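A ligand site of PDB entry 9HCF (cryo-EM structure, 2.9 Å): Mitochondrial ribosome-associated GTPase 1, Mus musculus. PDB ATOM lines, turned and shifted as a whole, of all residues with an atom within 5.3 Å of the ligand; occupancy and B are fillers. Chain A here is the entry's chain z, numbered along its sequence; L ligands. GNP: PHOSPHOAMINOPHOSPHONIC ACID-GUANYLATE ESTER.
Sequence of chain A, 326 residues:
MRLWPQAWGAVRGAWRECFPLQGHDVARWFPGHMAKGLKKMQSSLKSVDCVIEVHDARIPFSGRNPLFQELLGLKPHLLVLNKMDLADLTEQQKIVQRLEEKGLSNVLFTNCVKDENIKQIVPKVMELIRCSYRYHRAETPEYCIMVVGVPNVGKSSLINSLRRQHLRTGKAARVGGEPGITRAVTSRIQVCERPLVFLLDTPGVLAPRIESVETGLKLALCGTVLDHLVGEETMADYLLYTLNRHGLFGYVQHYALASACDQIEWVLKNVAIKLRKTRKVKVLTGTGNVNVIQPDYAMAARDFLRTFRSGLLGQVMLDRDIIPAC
OD1 of Asn 111 sits close to OD2 of Asp 85 (3.1 Å). N of Asn 111 lies close to SD of Met 84 (3.7 Å). The side-chain amide nitrogen of Asn 152 sits at hydrogen-bond distance from the backbone carbonyl oxygen of Gly 177 (2.5 Å). The backbone carbonyl oxygen of Pro 203 is in hydrogen-bond range of the side-chain amino group of Lys 155. The backbone carbonyl oxygen (O) of Thr 202 sits at hydrogen-bond distance from the side-chain amino group (NZ) of Lys 155 (3.2 Å). The backbone carbonyl oxygen (O) of Val 153 sits at hydrogen-bond distance from the side-chain amide nitrogen (ND2) of Asn 82 (3.0 Å). The backbone carbonyl oxygen (O) of Thr 110 sits close to the side-chain amide oxygen (OD1) of Asn 82, 2.7 Å away. OG1 of Thr 182 sits at hydrogen-bond distance from OD2 of Asp 201, 3.3 Å away.
O2A of the ligand is in hydrogen-bond range of N of Ser 157, at 2.7 Å. An oxygen (O2A) of the ligand lies within hydrogen-bond range of the side-chain hydroxyl (OG) of Ser 157 (2.5 Å). O6 of the ligand sits close to OD1 of Asn 111 (2.5 Å). The backbone NH (N) of Ser 156 sits at hydrogen-bond distance from an oxygen (O1B) of the ligand (2.5 Å). The side-chain hydroxyl (OG) of Ser 156 lies within hydrogen-bond range of an oxygen (O1B) of the ligand, 2.5 Å away. O1G of the ligand is in hydrogen-bond range of N of Asn 152. The backbone NH of Cys 112 is in hydrogen-bond range of an oxygen (O6) of the ligand, 2.8 Å away. O3G of the ligand lies close to N of Ile 181 (3.1 Å). O4' of the ligand is in hydrogen-bond range of NZ of Lys 83, at 3.2 Å. An oxygen (O3A) of the ligand lies within hydrogen-bond range of the backbone NH (N) of Lys 155 (3.2 Å). The side-chain amide nitrogen of Asn 82 sits at hydrogen-bond distance from a nitrogen (N7) of the ligand (3.2 Å). N of Thr 182 sits close to O3G of the ligand, 3.3 Å away. The backbone NH (N) of Val 153 is in hydrogen-bond range of an oxygen (O2B) of the ligand (3.3 Å). N of Gly 154 is in hydrogen-bond range of O3A of the ligand. A nitrogen (N2) of the ligand is in hydrogen-bond range of the side-chain carboxylate of Asp 85 (3.4 Å). O3G of the ligand sits at hydrogen-bond distance from N of Gly 180, at 3.5 Å.
An oxygen (O5') of the ligand sits close to the backbone carbonyl oxygen (O) of Gly 176 (3.3 Å). Leu 86 touches the ligand. CG2 of Val 113 touches N1 of the ligand, 3.5 Å away. O of Val 150 touches O2B of the ligand, 3.8 Å away. Pro 151 touches the ligand (CB to O1G, 3.2 Å). CG1 of Val 175 touches C5' of the ligand, 3.2 Å away. Gly 177 touches the ligand. CA of Pro 179 touches O1G of the ligand (3.5 Å). Gly 204 touches the ligand. Hydrophobic or aromatic side chains that line the ligand: Leu 86, Val 113, Pro 151, Val 153, Val 175 and Ile 181. Within 4 Å of the ligand: Asn 82, Lys 83, Asp 85, Leu 86, Asn 111, Cys 112, Val 113, Val 150, Pro 151, Asn 152, Val 153, Gly 154, Lys 155, Ser 156, Ser 157, Val 175, Gly 176, Gly 177, Pro 179, Gly 180, Ile 181, Thr 182 and Gly 204.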
ATOM      1  N   ASN A  82       5.934  10.690  24.279  1.00  0.00           N
ATOM      2  CA  ASN A  82       4.543  10.827  24.694  1.00  0.00           C
ATOM      3  C   ASN A  82       4.225   9.873  25.839  1.00  0.00           C
ATOM      4  O   ASN A  82       5.042   9.051  26.254  1.00  0.00           O
ATOM      5  CB  ASN A  82       3.607  10.562  23.513  1.00  0.00           C
ATOM      6  CG  ASN A  82       2.243  11.188  23.705  1.00  0.00           C
ATOM      7  OD1 ASN A  82       2.130  12.337  24.126  1.00  0.00           O
ATOM      8  ND2 ASN A  82       1.201  10.420  23.433  1.00  0.00           N
ATOM      9  N   LYS A  83       2.994  10.001  26.361  1.00  0.00           N
ATOM     10  CA  LYS A  83       2.516   9.160  27.456  1.00  0.00           C
ATOM     11  C   LYS A  83       3.382   9.321  28.707  1.00  0.00           C
ATOM     12  O   LYS A  83       3.660   8.351  29.413  1.00  0.00           O
ATOM     13  CB  LYS A  83       2.437   7.689  27.044  1.00  0.00           C
ATOM     14  CG  LYS A  83       1.326   7.376  26.051  1.00  0.00           C
ATOM     15  CD  LYS A  83       1.415   5.945  25.565  1.00  0.00           C
ATOM     16  CE  LYS A  83       0.447   5.669  24.422  1.00  0.00           C
ATOM     17  NZ  LYS A  83      -0.905   5.268  24.912  1.00  0.00           N
ATOM     18  N   MET A  84       3.806  10.555  28.979  1.00  0.00           N
ATOM     19  CA  MET A  84       4.655  10.818  30.138  1.00  0.00           C
ATOM     20  C   MET A  84       3.900  10.655  31.455  1.00  0.00           C
ATOM     21  O   MET A  84       4.536  10.428  32.487  1.00  0.00           O
ATOM     22  CB  MET A  84       5.241  12.226  30.048  1.00  0.00           C
ATOM     23  CG  MET A  84       4.212  13.333  30.090  1.00  0.00           C
ATOM     24  SD  MET A  84       4.945  14.961  29.866  1.00  0.00           S
ATOM     25  CE  MET A  84       5.753  15.195  31.454  1.00  0.00           C
ATOM     26  N   ASP A  85       2.572  10.783  31.448  1.00  0.00           N
ATOM     27  CA  ASP A  85       1.819  10.703  32.696  1.00  0.00           C
ATOM     28  C   ASP A  85       1.964   9.339  33.346  1.00  0.00           C
ATOM     29  O   ASP A  85       2.200   9.231  34.558  1.00  0.00           O
ATOM     30  CB  ASP A  85       0.342  11.016  32.440  1.00  0.00           C
ATOM     31  CG  ASP A  85      -0.250  10.187  31.320  1.00  0.00           C
ATOM     32  OD1 ASP A  85       0.523   9.479  30.637  1.00  0.00           O
ATOM     33  OD2 ASP A  85      -1.476  10.248  31.124  1.00  0.00           O
ATOM     34  N   LEU A  86       1.818   8.270  32.564  1.00  0.00           N
ATOM     35  CA  LEU A  86       1.948   6.911  33.095  1.00  0.00           C
ATOM     36  C   LEU A  86       3.375   6.382  32.946  1.00  0.00           C
ATOM     37  O   LEU A  86       3.624   5.292  32.429  1.00  0.00           O
ATOM     38  CB  LEU A  86       0.940   5.983  32.426  1.00  0.00           C
ATOM     39  CG  LEU A  86       1.120   5.544  30.963  1.00  0.00           C
ATOM     40  CD1 LEU A  86       0.236   4.344  30.684  1.00  0.00           C
ATOM     41  CD2 LEU A  86       0.786   6.664  30.010  1.00  0.00           C
ATOM     42  N   THR A 110       5.592  14.990  26.565  1.00  0.00           N
ATOM     43  CA  THR A 110       4.239  15.531  26.444  1.00  0.00           C
ATOM     44  C   THR A 110       3.207  14.471  26.769  1.00  0.00           C
ATOM     45  O   THR A 110       3.360  13.315  26.379  1.00  0.00           O
ATOM     46  CB  THR A 110       3.981  16.085  25.036  1.00  0.00           C
ATOM     47  OG1 THR A 110       3.852  14.998  24.114  1.00  0.00           O
ATOM     48  CG2 THR A 110       5.114  16.985  24.588  1.00  0.00           C
ATOM     49  N   ASN A 111       2.153  14.871  27.469  1.00  0.00           N
ATOM     50  CA  ASN A 111       0.992  14.024  27.733  1.00  0.00           C
ATOM     51  C   ASN A 111      -0.163  14.496  26.856  1.00  0.00           C
ATOM     52  O   ASN A 111      -0.703  15.591  27.069  1.00  0.00           O
ATOM     53  CB  ASN A 111       0.603  14.075  29.212  1.00  0.00           C
ATOM     54  CG  ASN A 111      -0.502  13.103  29.555  1.00  0.00           C
ATOM     55  OD1 ASN A 111      -0.754  12.154  28.812  1.00  0.00           O
ATOM     56  ND2 ASN A 111      -1.178  13.343  30.668  1.00  0.00           N
ATOM     57  N   CYS A 112      -0.534  13.686  25.863  1.00  0.00           N
ATOM     58  CA  CYS A 112      -1.568  14.107  24.925  1.00  0.00           C
ATOM     59  C   CYS A 112      -2.924  14.262  25.604  1.00  0.00           C
ATOM     60  O   CYS A 112      -3.624  15.252  25.366  1.00  0.00           O
ATOM     61  CB  CYS A 112      -1.675  13.099  23.776  1.00  0.00           C
ATOM     62  SG  CYS A 112      -0.273  13.133  22.638  1.00  0.00           S
ATOM     63  N   VAL A 113      -3.303  13.310  26.454  1.00  0.00           N
ATOM     64  CA  VAL A 113      -4.675  13.301  26.977  1.00  0.00           C
ATOM     65  C   VAL A 113      -4.967  14.567  27.779  1.00  0.00           C
ATOM     66  O   VAL A 113      -6.042  15.159  27.641  1.00  0.00           O
ATOM     67  CB  VAL A 113      -4.931  12.025  27.808  1.00  0.00           C
ATOM     68  CG1 VAL A 113      -5.008  10.813  26.894  1.00  0.00           C
ATOM     69  CG2 VAL A 113      -3.846  11.833  28.858  1.00  0.00           C
ATOM     70  N   VAL A 150       6.300   4.503  16.141  1.00  0.00           N
ATOM     71  CA  VAL A 150       5.779   3.143  16.260  1.00  0.00           C
ATOM     72  C   VAL A 150       4.308   3.214  16.680  1.00  0.00           C
ATOM     73  O   VAL A 150       3.863   4.239  17.199  1.00  0.00           O
ATOM     74  CB  VAL A 150       6.597   2.307  17.254  1.00  0.00           C
ATOM     75  CG1 VAL A 150       8.032   2.178  16.772  1.00  0.00           C
ATOM     76  CG2 VAL A 150       6.562   2.915  18.648  1.00  0.00           C
ATOM     77  N   PRO A 151       3.534   2.144  16.481  1.00  0.00           N
ATOM     78  CA  PRO A 151       2.093   2.208  16.776  1.00  0.00           C
ATOM     79  C   PRO A 151       1.796   2.461  18.245  1.00  0.00           C
ATOM     80  O   PRO A 151       2.560   2.082  19.139  1.00  0.00           O
ATOM     81  CB  PRO A 151       1.584   0.830  16.334  1.00  0.00           C
ATOM     82  CG  PRO A 151       2.583   0.363  15.335  1.00  0.00           C
ATOM     83  CD  PRO A 151       3.892   0.879  15.816  1.00  0.00           C
ATOM     84  N   ASN A 152       0.660   3.119  18.493  1.00  0.00           N
ATOM     85  CA  ASN A 152       0.152   3.384  19.839  1.00  0.00           C
ATOM     86  C   ASN A 152       1.150   4.150  20.694  1.00  0.00           C
ATOM     87  O   ASN A 152       1.406   3.797  21.850  1.00  0.00           O
ATOM     88  CB  ASN A 152      -0.266   2.087  20.552  1.00  0.00           C
ATOM     89  CG  ASN A 152      -1.484   1.455  19.926  1.00  0.00           C
ATOM     90  OD1 ASN A 152      -1.428   0.325  19.448  1.00  0.00           O
ATOM     91  ND2 ASN A 152      -2.602   2.173  19.923  1.00  0.00           N
ATOM     92  N   VAL A 153       1.729   5.207  20.128  1.00  0.00           N
ATOM     93  CA  VAL A 153       2.546   6.141  20.879  1.00  0.00           C
ATOM     94  C   VAL A 153       1.850   7.480  21.059  1.00  0.00           C
ATOM     95  O   VAL A 153       2.453   8.436  21.551  1.00  0.00           O
ATOM     96  CB  VAL A 153       3.928   6.325  20.228  1.00  0.00           C
ATOM     97  CG1 VAL A 153       4.679   5.019  20.227  1.00  0.00           C
ATOM     98  CG2 VAL A 153       3.786   6.877  18.825  1.00  0.00           C
ATOM     99  N   GLY A 154       0.583   7.584  20.664  1.00  0.00           N
ATOM    100  CA  GLY A 154      -0.103   8.851  20.655  1.00  0.00           C
ATOM    101  C   GLY A 154       0.147   9.674  19.413  1.00  0.00           C
ATOM    102  O   GLY A 154      -0.138  10.875  19.418  1.00  0.00           O
ATOM    103  N   LYS A 155       0.671   9.060  18.356  1.00  0.00           N
ATOM    104  CA  LYS A 155       1.011   9.801  17.152  1.00  0.00           C
ATOM    105  C   LYS A 155      -0.218  10.495  16.561  1.00  0.00           C
ATOM    106  O   LYS A 155      -0.160  11.676  16.206  1.00  0.00           O
ATOM    107  CB  LYS A 155       1.643   8.851  16.141  1.00  0.00           C
ATOM    108  CG  LYS A 155       2.105   9.482  14.848  1.00  0.00           C
ATOM    109  CD  LYS A 155       2.194   8.440  13.749  1.00  0.00           C
ATOM    110  CE  LYS A 155       3.098   7.296  14.157  1.00  0.00           C
ATOM    111  NZ  LYS A 155       3.502   6.483  12.990  1.00  0.00           N
ATOM    112  N   SER A 156      -1.330   9.765  16.443  1.00  0.00           N
ATOM    113  CA  SER A 156      -2.544  10.367  15.931  1.00  0.00           C
ATOM    114  C   SER A 156      -3.126  11.357  16.943  1.00  0.00           C
ATOM    115  O   SER A 156      -3.685  12.394  16.556  1.00  0.00           O
ATOM    116  CB  SER A 156      -3.568   9.284  15.594  1.00  0.00           C
ATOM    117  OG  SER A 156      -3.039   8.367  14.653  1.00  0.00           O
ATOM    118  N   SER A 157      -3.007  11.052  18.238  1.00  0.00           N
ATOM    119  CA  SER A 157      -3.515  11.960  19.262  1.00  0.00           C
ATOM    120  C   SER A 157      -2.791  13.294  19.214  1.00  0.00           C
ATOM    121  O   SER A 157      -3.408  14.354  19.365  1.00  0.00           O
ATOM    122  CB  SER A 157      -3.388  11.326  20.641  1.00  0.00           C
ATOM    123  OG  SER A 157      -4.259  10.222  20.767  1.00  0.00           O
ATOM    124  N   LEU A 158      -1.467  13.277  19.021  1.00  0.00           N
ATOM    125  CA  LEU A 158      -0.710  14.514  18.972  1.00  0.00           C
ATOM    126  C   LEU A 158      -1.270  15.463  17.937  1.00  0.00           C
ATOM    127  O   LEU A 158      -1.239  16.691  18.127  1.00  0.00           O
ATOM    128  CB  LEU A 158       0.769  14.210  18.678  1.00  0.00           C
ATOM    129  CG  LEU A 158       1.745  15.375  18.823  1.00  0.00           C
ATOM    130  CD1 LEU A 158       3.115  14.867  19.227  1.00  0.00           C
ATOM    131  CD2 LEU A 158       1.844  16.180  17.526  1.00  0.00           C
ATOM    132  N   ARG A 174      -8.547   9.885  13.782  1.00  0.00           N
ATOM    133  CA  ARG A 174      -9.207   8.833  14.563  1.00  0.00           C
ATOM    134  C   ARG A 174      -8.220   8.252  15.562  1.00  0.00           C
ATOM    135  O   ARG A 174      -7.217   7.651  15.189  1.00  0.00           O
ATOM    136  CB  ARG A 174      -9.756   7.755  13.649  1.00  0.00           C
ATOM    137  CG  ARG A 174     -10.505   6.663  14.383  1.00  0.00           C
ATOM    138  CD  ARG A 174     -11.250   5.741  13.427  1.00  0.00           C
ATOM    139  NE  ARG A 174     -12.495   6.331  12.967  1.00  0.00           N
ATOM    140  CZ  ARG A 174     -13.204   5.890  11.930  1.00  0.00           C
ATOM    141  NH1 ARG A 174     -12.802   4.844  11.219  1.00  0.00           N
ATOM    142  NH2 ARG A 174     -14.342   6.496  11.620  1.00  0.00           N
ATOM    143  N   VAL A 175      -8.514   8.430  16.849  1.00  0.00           N
ATOM    144  CA  VAL A 175      -7.663   7.994  17.950  1.00  0.00           C
ATOM    145  C   VAL A 175      -8.251   6.711  18.508  1.00  0.00           C
ATOM    146  O   VAL A 175      -9.423   6.675  18.896  1.00  0.00           O
ATOM    147  CB  VAL A 175      -7.551   9.074  19.030  1.00  0.00           C
ATOM    148  CG1 VAL A 175      -6.658   8.613  20.146  1.00  0.00           C
ATOM    149  CG2 VAL A 175      -7.017  10.365  18.427  1.00  0.00           C
ATOM    150  N   GLY A 176      -7.449   5.654  18.557  1.00  0.00           N
ATOM    151  CA  GLY A 176      -7.913   4.360  18.989  1.00  0.00           C
ATOM    152  C   GLY A 176      -6.898   3.668  19.870  1.00  0.00           C
ATOM    153  O   GLY A 176      -5.696   3.920  19.788  1.00  0.00           O
ATOM    154  N   GLY A 177      -7.402   2.766  20.723  1.00  0.00           N
ATOM    155  CA  GLY A 177      -6.528   2.073  21.645  1.00  0.00           C
ATOM    156  C   GLY A 177      -5.631   1.047  20.974  1.00  0.00           C
ATOM    157  O   GLY A 177      -4.417   1.021  21.197  1.00  0.00           O
ATOM    158  N   GLU A 178      -6.215   0.188  20.135  1.00  0.00           N
ATOM    159  CA  GLU A 178      -5.459  -0.933  19.585  1.00  0.00           C
ATOM    160  C   GLU A 178      -4.589  -0.484  18.412  1.00  0.00           C
ATOM    161  O   GLU A 178      -4.967   0.432  17.671  1.00  0.00           O
ATOM    162  CB  GLU A 178      -6.418  -2.050  19.144  1.00  0.00           C
ATOM    163  CG  GLU A 178      -6.967  -1.915  17.727  1.00  0.00           C
ATOM    164  CD  GLU A 178      -7.871  -3.075  17.361  1.00  0.00           C
ATOM    165  OE1 GLU A 178      -8.044  -3.979  18.200  1.00  0.00           O
ATOM    166  OE2 GLU A 178      -8.414  -3.075  16.233  1.00  0.00           O
ATOM    167  N   PRO A 179      -3.429  -1.103  18.210  1.00  0.00           N
ATOM    168  CA  PRO A 179      -2.553  -0.704  17.108  1.00  0.00           C
ATOM    169  C   PRO A 179      -3.168  -0.978  15.741  1.00  0.00           C
ATOM    170  O   PRO A 179      -3.967  -1.901  15.564  1.00  0.00           O
ATOM    171  CB  PRO A 179      -1.290  -1.551  17.318  1.00  0.00           C
ATOM    172  CG  PRO A 179      -1.748  -2.724  18.116  1.00  0.00           C
ATOM    173  CD  PRO A 179      -2.841  -2.206  19.007  1.00  0.00           C
ATOM    174  N   GLY A 180      -2.794  -0.153  14.768  1.00  0.00           N
ATOM    175  CA  GLY A 180      -3.213  -0.320  13.399  1.00  0.00           C
ATOM    176  C   GLY A 180      -4.393   0.514  12.959  1.00  0.00           C
ATOM    177  O   GLY A 180      -4.914   0.288  11.863  1.00  0.00           O
ATOM    178  N   ILE A 181      -4.836   1.473  13.783  1.00  0.00           N
ATOM    179  CA  ILE A 181      -6.028   2.240  13.435  1.00  0.00           C
ATOM    180  C   ILE A 181      -5.765   3.115  12.205  1.00  0.00           C
ATOM    181  O   ILE A 181      -6.576   3.152  11.277  1.00  0.00           O
ATOM    182  CB  ILE A 181      -6.500   3.088  14.633  1.00  0.00           C
ATOM    183  CG1 ILE A 181      -5.351   3.947  15.174  1.00  0.00           C
ATOM    184  CG2 ILE A 181      -7.032   2.186  15.732  1.00  0.00           C
ATOM    185  CD1 ILE A 181      -5.786   4.929  16.201  1.00  0.00           C
ATOM    186  N   THR A 182      -4.633   3.809  12.181  1.00  0.00           N
ATOM    187  CA  THR A 182      -4.282   4.664  11.049  1.00  0.00           C
ATOM    188  C   THR A 182      -3.414   3.859  10.095  1.00  0.00           C
ATOM    189  O   THR A 182      -2.333   3.388  10.463  1.00  0.00           O
ATOM    190  CB  THR A 182      -3.558   5.933  11.508  1.00  0.00           C
ATOM    191  OG1 THR A 182      -3.170   6.703  10.368  1.00  0.00           O
ATOM    192  CG2 THR A 182      -2.325   5.613  12.349  1.00  0.00           C
ATOM    193  N   ASP A 201       0.007  12.819   8.906  1.00  0.00           N
ATOM    194  CA  ASP A 201      -0.122  11.643   9.769  1.00  0.00           C
ATOM    195  C   ASP A 201       0.162  10.384   8.976  1.00  0.00           C
ATOM    196  O   ASP A 201      -0.315  10.223   7.842  1.00  0.00           O
ATOM    197  CB  ASP A 201      -1.512  11.574  10.393  1.00  0.00           C
ATOM    198  CG  ASP A 201      -1.750  10.291  11.158  1.00  0.00           C
ATOM    199  OD1 ASP A 201      -0.760   9.671  11.593  1.00  0.00           O
ATOM    200  OD2 ASP A 201      -2.921   9.898  11.319  1.00  0.00           O
ATOM    201  N   THR A 202       0.926   9.476   9.563  1.00  0.00           N
ATOM    202  CA  THR A 202       1.403   8.271   8.911  1.00  0.00           C
ATOM    203  C   THR A 202       1.181   7.056   9.791  1.00  0.00           C
ATOM    204  O   THR A 202       1.080   7.185  11.012  1.00  0.00           O
ATOM    205  CB  THR A 202       2.894   8.388   8.564  1.00  0.00           C
ATOM    206  OG1 THR A 202       3.662   8.405   9.769  1.00  0.00           O
ATOM    207  CG2 THR A 202       3.162   9.659   7.781  1.00  0.00           C
ATOM    208  N   PRO A 203       1.098   5.867   9.202  1.00  0.00           N
ATOM    209  CA  PRO A 203       0.916   4.648  10.007  1.00  0.00           C
ATOM    210  C   PRO A 203       2.159   4.295  10.807  1.00  0.00           C
ATOM    211  O   PRO A 203       3.292   4.536  10.378  1.00  0.00           O
ATOM    212  CB  PRO A 203       0.616   3.582   8.959  1.00  0.00           C
ATOM    213  CG  PRO A 203       1.318   4.071   7.734  1.00  0.00           C
ATOM    214  CD  PRO A 203       1.134   5.553   7.761  1.00  0.00           C
ATOM    215  N   GLY A 204       1.935   3.703  11.978  1.00  0.00           N
ATOM    216  CA  GLY A 204       3.019   3.253  12.828  1.00  0.00           C
ATOM    217  C   GLY A 204       3.829   2.131  12.216  1.00  0.00           C
ATOM    218  O   GLY A 204       3.264   1.136  11.759  1.00  0.00           O
HETATM  219  PG  GNP L   1      -1.435   3.612  15.679  1.00  0.00           P
HETATM  220  O1G GNP L   1      -1.142   2.408  16.531  1.00  0.00           O
HETATM  221  O2G GNP L   1      -0.196   3.983  14.908  1.00  0.00           O
HETATM  222  O3G GNP L   1      -2.563   3.329  14.734  1.00  0.00           O
HETATM  223  N3B GNP L   1      -1.888   4.885  16.589  1.00  0.00           N
HETATM  224  PB  GNP L   1      -1.033   6.206  16.987  1.00  0.00           P
HETATM  225  O1B GNP L   1      -1.174   7.275  15.982  1.00  0.00           O
HETATM  226  O2B GNP L   1       0.387   5.863  17.172  1.00  0.00           O
HETATM  227  O3A GNP L   1      -1.623   6.863  18.299  1.00  0.00           O
HETATM  228  PA  GNP L   1      -3.103   7.173  18.823  1.00  0.00           P
HETATM  229  O1A GNP L   1      -4.067   6.756  17.803  1.00  0.00           O
HETATM  230  O2A GNP L   1      -3.136   8.573  19.306  1.00  0.00           O
HETATM  231  O5' GNP L   1      -3.276   6.208  20.076  1.00  0.00           O
HETATM  232  C5' GNP L   1      -4.425   6.427  20.911  1.00  0.00           C
HETATM  233  C4' GNP L   1      -4.418   5.523  22.107  1.00  0.00           C
HETATM  234  O4' GNP L   1      -3.333   5.899  22.989  1.00  0.00           O
HETATM  235  C3' GNP L   1      -5.668   5.628  22.971  1.00  0.00           C
HETATM  236  O3' GNP L   1      -5.843   4.437  23.735  1.00  0.00           O
HETATM  237  C2' GNP L   1      -5.321   6.817  23.866  1.00  0.00           C
HETATM  238  O2' GNP L   1      -6.094   6.906  25.053  1.00  0.00           O
HETATM  239  C1' GNP L   1      -3.849   6.507  24.159  1.00  0.00           C
HETATM  240  N9  GNP L   1      -3.043   7.703  24.451  1.00  0.00           N
HETATM  241  C8  GNP L   1      -2.527   8.603  23.554  1.00  0.00           C
HETATM  242  N7  GNP L   1      -1.847   9.560  24.126  1.00  0.00           N
HETATM  243  C5  GNP L   1      -1.923   9.274  25.476  1.00  0.00           C
HETATM  244  C6  GNP L   1      -1.380   9.947  26.630  1.00  0.00           C
HETATM  245  O6  GNP L   1      -0.699  10.967  26.573  1.00  0.00           O
HETATM  246  N1  GNP L   1      -1.676   9.345  27.777  1.00  0.00           N
HETATM  247  C2  GNP L   1      -2.424   8.201  27.902  1.00  0.00           C
HETATM  248  N2  GNP L   1      -2.627   7.747  29.133  1.00  0.00           N
HETATM  249  N3  GNP L   1      -2.951   7.555  26.865  1.00  0.00           N
HETATM  250  C4  GNP L   1      -2.660   8.139  25.694  1.00  0.00           C
